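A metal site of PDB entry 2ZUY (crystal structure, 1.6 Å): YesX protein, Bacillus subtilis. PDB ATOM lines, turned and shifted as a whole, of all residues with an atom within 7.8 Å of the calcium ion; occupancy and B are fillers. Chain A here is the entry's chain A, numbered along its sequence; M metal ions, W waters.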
ATOM      1  N   HIS A 424      -8.620   5.035   1.518  1.00  0.00           N
ATOM      2  CA  HIS A 424      -8.060   4.085   2.466  1.00  0.00           C
ATOM      3  C   HIS A 424      -6.873   4.741   3.181  1.00  0.00           C
ATOM      4  O   HIS A 424      -5.729   4.702   2.719  1.00  0.00           O
ATOM      5  CB  HIS A 424      -7.668   2.782   1.748  1.00  0.00           C
ATOM      6  CG  HIS A 424      -6.992   1.778   2.617  1.00  0.00           C
ATOM      7  ND1 HIS A 424      -7.648   1.042   3.572  1.00  0.00           N
ATOM      8  CD2 HIS A 424      -5.686   1.379   2.663  1.00  0.00           C
ATOM      9  CE1 HIS A 424      -6.791   0.241   4.183  1.00  0.00           C
ATOM     10  NE2 HIS A 424      -5.596   0.415   3.643  1.00  0.00           N
ATOM     11  N   ILE A 469      -3.995  10.985  -2.939  1.00  0.00           N
ATOM     12  CA  ILE A 469      -2.889  10.677  -3.844  1.00  0.00           C
ATOM     13  C   ILE A 469      -2.061   9.505  -3.296  1.00  0.00           C
ATOM     14  O   ILE A 469      -1.766   9.468  -2.110  1.00  0.00           O
ATOM     15  CB  ILE A 469      -1.986  11.923  -4.089  1.00  0.00           C
ATOM     16  CG1 ILE A 469      -0.926  11.638  -5.158  1.00  0.00           C
ATOM     17  CG2 ILE A 469      -1.336  12.431  -2.792  1.00  0.00           C
ATOM     18  CD1 ILE A 469      -0.166  12.871  -5.640  1.00  0.00           C
ATOM     19  N   TRP A 470      -1.720   8.549  -4.161  1.00  0.00           N
ATOM     20  CA  TRP A 470      -0.727   7.526  -3.800  1.00  0.00           C
ATOM     21  C   TRP A 470       0.647   8.118  -4.024  1.00  0.00           C
ATOM     22  O   TRP A 470       1.087   8.291  -5.187  1.00  0.00           O
ATOM     23  CB  TRP A 470      -0.916   6.227  -4.596  1.00  0.00           C
ATOM     24  CG  TRP A 470      -2.174   5.497  -4.209  1.00  0.00           C
ATOM     25  CD1 TRP A 470      -2.429   4.888  -3.016  1.00  0.00           C
ATOM     26  CD2 TRP A 470      -3.347   5.323  -5.013  1.00  0.00           C
ATOM     27  NE1 TRP A 470      -3.693   4.332  -3.026  1.00  0.00           N
ATOM     28  CE2 TRP A 470      -4.273   4.589  -4.240  1.00  0.00           C
ATOM     29  CE3 TRP A 470      -3.701   5.709  -6.319  1.00  0.00           C
ATOM     30  CZ2 TRP A 470      -5.544   4.236  -4.723  1.00  0.00           C
ATOM     31  CZ3 TRP A 470      -4.964   5.360  -6.807  1.00  0.00           C
ATOM     32  CH2 TRP A 470      -5.875   4.632  -6.007  1.00  0.00           C
ATOM     33  N   TRP A 471       1.312   8.436  -2.920  1.00  0.00           N
ATOM     34  CA  TRP A 471       2.565   9.206  -2.962  1.00  0.00           C
ATOM     35  C   TRP A 471       3.767   8.445  -2.431  1.00  0.00           C
ATOM     36  O   TRP A 471       4.819   8.410  -3.064  1.00  0.00           O
ATOM     37  CB  TRP A 471       2.406  10.526  -2.216  1.00  0.00           C
ATOM     38  CG  TRP A 471       3.642  11.401  -2.285  1.00  0.00           C
ATOM     39  CD1 TRP A 471       4.468  11.723  -1.249  1.00  0.00           C
ATOM     40  CD2 TRP A 471       4.193  12.019  -3.459  1.00  0.00           C
ATOM     41  NE1 TRP A 471       5.498  12.528  -1.704  1.00  0.00           N
ATOM     42  CE2 TRP A 471       5.354  12.724  -3.052  1.00  0.00           C
ATOM     43  CE3 TRP A 471       3.819  12.055  -4.818  1.00  0.00           C
ATOM     44  CZ2 TRP A 471       6.149  13.447  -3.948  1.00  0.00           C
ATOM     45  CZ3 TRP A 471       4.597  12.783  -5.698  1.00  0.00           C
ATOM     46  CH2 TRP A 471       5.744  13.473  -5.264  1.00  0.00           C
ATOM     47  N   ASP A 472       3.631   7.869  -1.232  1.00  0.00           N
ATOM     48  CA  ASP A 472       4.750   7.110  -0.668  1.00  0.00           C
ATOM     49  C   ASP A 472       4.676   5.625  -1.070  1.00  0.00           C
ATOM     50  O   ASP A 472       3.975   5.274  -2.020  1.00  0.00           O
ATOM     51  CB  ASP A 472       4.868   7.341   0.855  1.00  0.00           C
ATOM     52  CG  ASP A 472       3.683   6.792   1.634  1.00  0.00           C
ATOM     53  OD1 ASP A 472       3.509   7.200   2.804  1.00  0.00           O
ATOM     54  OD2 ASP A 472       2.939   5.941   1.098  1.00  0.00           O
ATOM     55  N   GLY A 473       5.389   4.769  -0.346  1.00  0.00           N
ATOM     56  CA  GLY A 473       5.517   3.368  -0.755  1.00  0.00           C
ATOM     57  C   GLY A 473       4.435   2.421  -0.286  1.00  0.00           C
ATOM     58  O   GLY A 473       4.352   1.291  -0.769  1.00  0.00           O
ATOM     59  N   ASP A 474       3.603   2.855   0.668  1.00  0.00           N
ATOM     60  CA  ASP A 474       2.614   1.926   1.247  1.00  0.00           C
ATOM     61  C   ASP A 474       1.245   1.983   0.554  1.00  0.00           C
ATOM     62  O   ASP A 474       0.981   2.875  -0.253  1.00  0.00           O
ATOM     63  CB  ASP A 474       2.520   2.063   2.776  1.00  0.00           C
ATOM     64  CG  ASP A 474       1.814   3.340   3.226  1.00  0.00           C
ATOM     65  OD1 ASP A 474       1.951   3.696   4.430  1.00  0.00           O
ATOM     66  OD2 ASP A 474       1.109   3.995   2.427  1.00  0.00           O
ATOM     67  N   LEU A 475       0.384   1.029   0.901  1.00  0.00           N
ATOM     68  CA  LEU A 475      -0.921   0.874   0.225  1.00  0.00           C
ATOM     69  C   LEU A 475      -1.974   1.896   0.654  1.00  0.00           C
ATOM     70  O   LEU A 475      -2.960   2.087  -0.052  1.00  0.00           O
ATOM     71  CB  LEU A 475      -1.462  -0.550   0.408  1.00  0.00           C
ATOM     72  CG  LEU A 475      -0.631  -1.684  -0.196  1.00  0.00           C
ATOM     73  CD1 LEU A 475      -1.249  -3.025   0.166  1.00  0.00           C
ATOM     74  CD2 LEU A 475      -0.499  -1.530  -1.707  1.00  0.00           C
ATOM     75  N   VAL A 476      -1.741   2.547   1.790  1.00  0.00           N
ATOM     76  CA  VAL A 476      -2.602   3.631   2.239  1.00  0.00           C
ATOM     77  C   VAL A 476      -2.492   4.786   1.230  1.00  0.00           C
ATOM     78  O   VAL A 476      -1.448   4.967   0.590  1.00  0.00           O
ATOM     79  CB  VAL A 476      -2.217   4.070   3.672  1.00  0.00           C
ATOM     80  CG1 VAL A 476      -2.542   5.539   3.919  1.00  0.00           C
ATOM     81  CG2 VAL A 476      -2.908   3.153   4.692  1.00  0.00           C
ATOM     82  N   ARG A 477      -3.587   5.529   1.053  1.00  0.00           N
ATOM     83  CA  ARG A 477      -3.539   6.709   0.201  1.00  0.00           C
ATOM     84  C   ARG A 477      -3.272   7.961   1.040  1.00  0.00           C
ATOM     85  O   ARG A 477      -3.807   8.104   2.141  1.00  0.00           O
ATOM     86  CB  ARG A 477      -4.826   6.861  -0.627  1.00  0.00           C
ATOM     87  CG  ARG A 477      -4.591   7.563  -1.973  1.00  0.00           C
ATOM     88  CD  ARG A 477      -5.795   7.443  -2.915  1.00  0.00           C
ATOM     89  NE  ARG A 477      -5.469   7.950  -4.251  1.00  0.00           N
ATOM     90  CZ  ARG A 477      -6.353   8.241  -5.213  1.00  0.00           C
ATOM     91  NH1 ARG A 477      -7.658   8.078  -4.998  1.00  0.00           N
ATOM     92  NH2 ARG A 477      -5.926   8.687  -6.387  1.00  0.00           N
ATOM     93  N   GLU A 478      -2.430   8.827   0.507  1.00  0.00           N
ATOM     94  CA  GLU A 478      -2.091  10.089   1.153  1.00  0.00           C
ATOM     95  C   GLU A 478      -3.103  11.153   0.717  1.00  0.00           C
ATOM     96  O   GLU A 478      -3.972  10.890  -0.128  1.00  0.00           O
ATOM     97  CB  GLU A 478      -0.646  10.481   0.791  1.00  0.00           C
ATOM     98  CG  GLU A 478       0.416   9.641   1.519  1.00  0.00           C
ATOM     99  CD  GLU A 478       0.438   8.155   1.104  1.00  0.00           C
ATOM    100  OE1 GLU A 478       0.771   7.833  -0.058  1.00  0.00           O
ATOM    101  OE2 GLU A 478       0.168   7.287   1.972  1.00  0.00           O
ATOM    102  N   LYS A 495      -0.174  12.906   5.414  1.00  0.00           N
ATOM    103  CA  LYS A 495      -0.468  11.508   5.711  1.00  0.00           C
ATOM    104  C   LYS A 495      -1.239  11.408   7.018  1.00  0.00           C
ATOM    105  O   LYS A 495      -0.909  12.071   7.998  1.00  0.00           O
ATOM    106  CB  LYS A 495       0.811  10.677   5.787  1.00  0.00           C
ATOM    107  CG  LYS A 495       0.556   9.190   5.656  1.00  0.00           C
ATOM    108  CD  LYS A 495       1.840   8.400   5.731  1.00  0.00           C
ATOM    109  CE  LYS A 495       1.554   6.906   5.702  1.00  0.00           C
ATOM    110  NZ  LYS A 495       1.360   6.413   4.317  1.00  0.00           N
ATOM    111  N   ILE A 506       3.935  15.610   4.671  1.00  0.00           N
ATOM    112  CA  ILE A 506       5.050  14.804   4.145  1.00  0.00           C
ATOM    113  C   ILE A 506       5.693  15.371   2.876  1.00  0.00           C
ATOM    114  O   ILE A 506       6.766  14.915   2.466  1.00  0.00           O
ATOM    115  CB  ILE A 506       4.660  13.312   3.927  1.00  0.00           C
ATOM    116  CG1 ILE A 506       3.527  13.190   2.895  1.00  0.00           C
ATOM    117  CG2 ILE A 506       4.310  12.654   5.271  1.00  0.00           C
ATOM    118  CD1 ILE A 506       3.196  11.754   2.499  1.00  0.00           C
ATOM    119  N   TRP A 532       3.472   2.959 -10.297  1.00  0.00           N
ATOM    120  CA  TRP A 532       2.054   3.242 -10.075  1.00  0.00           C
ATOM    121  C   TRP A 532       1.756   4.456  -9.189  1.00  0.00           C
ATOM    122  O   TRP A 532       0.618   4.924  -9.171  1.00  0.00           O
ATOM    123  CB  TRP A 532       1.358   2.002  -9.505  1.00  0.00           C
ATOM    124  CG  TRP A 532       1.938   1.529  -8.221  1.00  0.00           C
ATOM    125  CD1 TRP A 532       2.992   0.678  -8.065  1.00  0.00           C
ATOM    126  CD2 TRP A 532       1.500   1.884  -6.901  1.00  0.00           C
ATOM    127  NE1 TRP A 532       3.240   0.478  -6.722  1.00  0.00           N
ATOM    128  CE2 TRP A 532       2.338   1.202  -5.984  1.00  0.00           C
ATOM    129  CE3 TRP A 532       0.465   2.701  -6.402  1.00  0.00           C
ATOM    130  CZ2 TRP A 532       2.186   1.311  -4.598  1.00  0.00           C
ATOM    131  CZ3 TRP A 532       0.314   2.810  -5.016  1.00  0.00           C
ATOM    132  CH2 TRP A 532       1.173   2.122  -4.129  1.00  0.00           C
ATOM    133  N   ARG A 533       2.740   4.966  -8.455  1.00  0.00           N
ATOM    134  CA  ARG A 533       2.508   6.182  -7.682  1.00  0.00           C
ATOM    135  C   ARG A 533       2.193   7.354  -8.610  1.00  0.00           C
ATOM    136  O   ARG A 533       2.588   7.371  -9.778  1.00  0.00           O
ATOM    137  CB  ARG A 533       3.698   6.529  -6.786  1.00  0.00           C
ATOM    138  CG  ARG A 533       3.606   5.916  -5.378  1.00  0.00           C
ATOM    139  CD  ARG A 533       3.885   4.412  -5.356  1.00  0.00           C
ATOM    140  NE  ARG A 533       5.229   4.094  -5.844  1.00  0.00           N
ATOM    141  CZ  ARG A 533       6.346   4.231  -5.129  1.00  0.00           C
ATOM    142  NH1 ARG A 533       6.305   4.688  -3.883  1.00  0.00           N
ATOM    143  NH2 ARG A 533       7.513   3.909  -5.688  1.00  0.00           N
ATOM    144  N   THR A 555       8.855   1.292  -3.014  1.00  0.00           N
ATOM    145  CA  THR A 555       7.672   0.479  -2.710  1.00  0.00           C
ATOM    146  C   THR A 555       8.022  -0.988  -2.920  1.00  0.00           C
ATOM    147  O   THR A 555       8.908  -1.319  -3.722  1.00  0.00           O
ATOM    148  CB  THR A 555       6.423   0.875  -3.555  1.00  0.00           C
ATOM    149  OG1 THR A 555       5.267   0.173  -3.092  1.00  0.00           O
ATOM    150  CG2 THR A 555       6.640   0.572  -5.043  1.00  0.00           C
ATOM    151  N   LEU A 589      -7.600  -0.799  -4.112  1.00  0.00           N
ATOM    152  CA  LEU A 589      -6.163  -0.704  -3.858  1.00  0.00           C
ATOM    153  C   LEU A 589      -6.009  -0.318  -2.399  1.00  0.00           C
ATOM    154  O   LEU A 589      -6.407   0.772  -1.998  1.00  0.00           O
ATOM    155  CB  LEU A 589      -5.523   0.353  -4.777  1.00  0.00           C
ATOM    156  CG  LEU A 589      -3.991   0.324  -4.992  1.00  0.00           C
ATOM    157  CD1 LEU A 589      -3.620   1.198  -6.185  1.00  0.00           C
ATOM    158  CD2 LEU A 589      -3.205   0.740  -3.736  1.00  0.00           C
HETATM  159 CA    CA M   1       0.799   5.365   0.562  1.00  0.00          CA
HETATM  160  O   HOH W   1       1.211   5.196  -1.845  1.00  0.00           O
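The side-chain carboxylate (OD1) of Asp 474 lies within salt-bridge range of the side-chain amino group (NZ) of Lys 495, at 2.8 Å. NH1 of Arg 533 lies within hydrogen-bond range of O of Asp 472, 3.0 Å away. The side-chain amino group of Lys 495 is in salt-bridge range of the side-chain carboxylate of Asp 472, at 2.7 Å. N of Glu 478 is in hydrogen-bond range of O of Ile 469 (2.8 Å). The side-chain carboxylate (OE2) of Glu 478 sits close to the side-chain amino group (NZ) of Lys 495 (2.8 Å). OE1 of Glu 478 lies close to N of Trp 471, 3.0 Å away.
OD2 of Asp 472 is bound to the calcium ion, at 2.3 Å. The backbone carbonyl oxygen (O) of Val 476 binds the calcium ion, at 2.3 Å. The side-chain carboxylate (OD2) of Asp 474 is bound to the calcium ion. Water W1 is bound to the calcium ion. The side-chain carboxylate (OE2) of Glu 478 binds the calcium ion, at 2.5 Å. OE1 of Glu 478 binds the calcium ion, 2.5 Å away. O of Asp 474 is bound to the calcium ion, at 2.6 Å. The calcium ion has seven donor atoms within binding distance.
Lys 495 touches the calcium ion.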
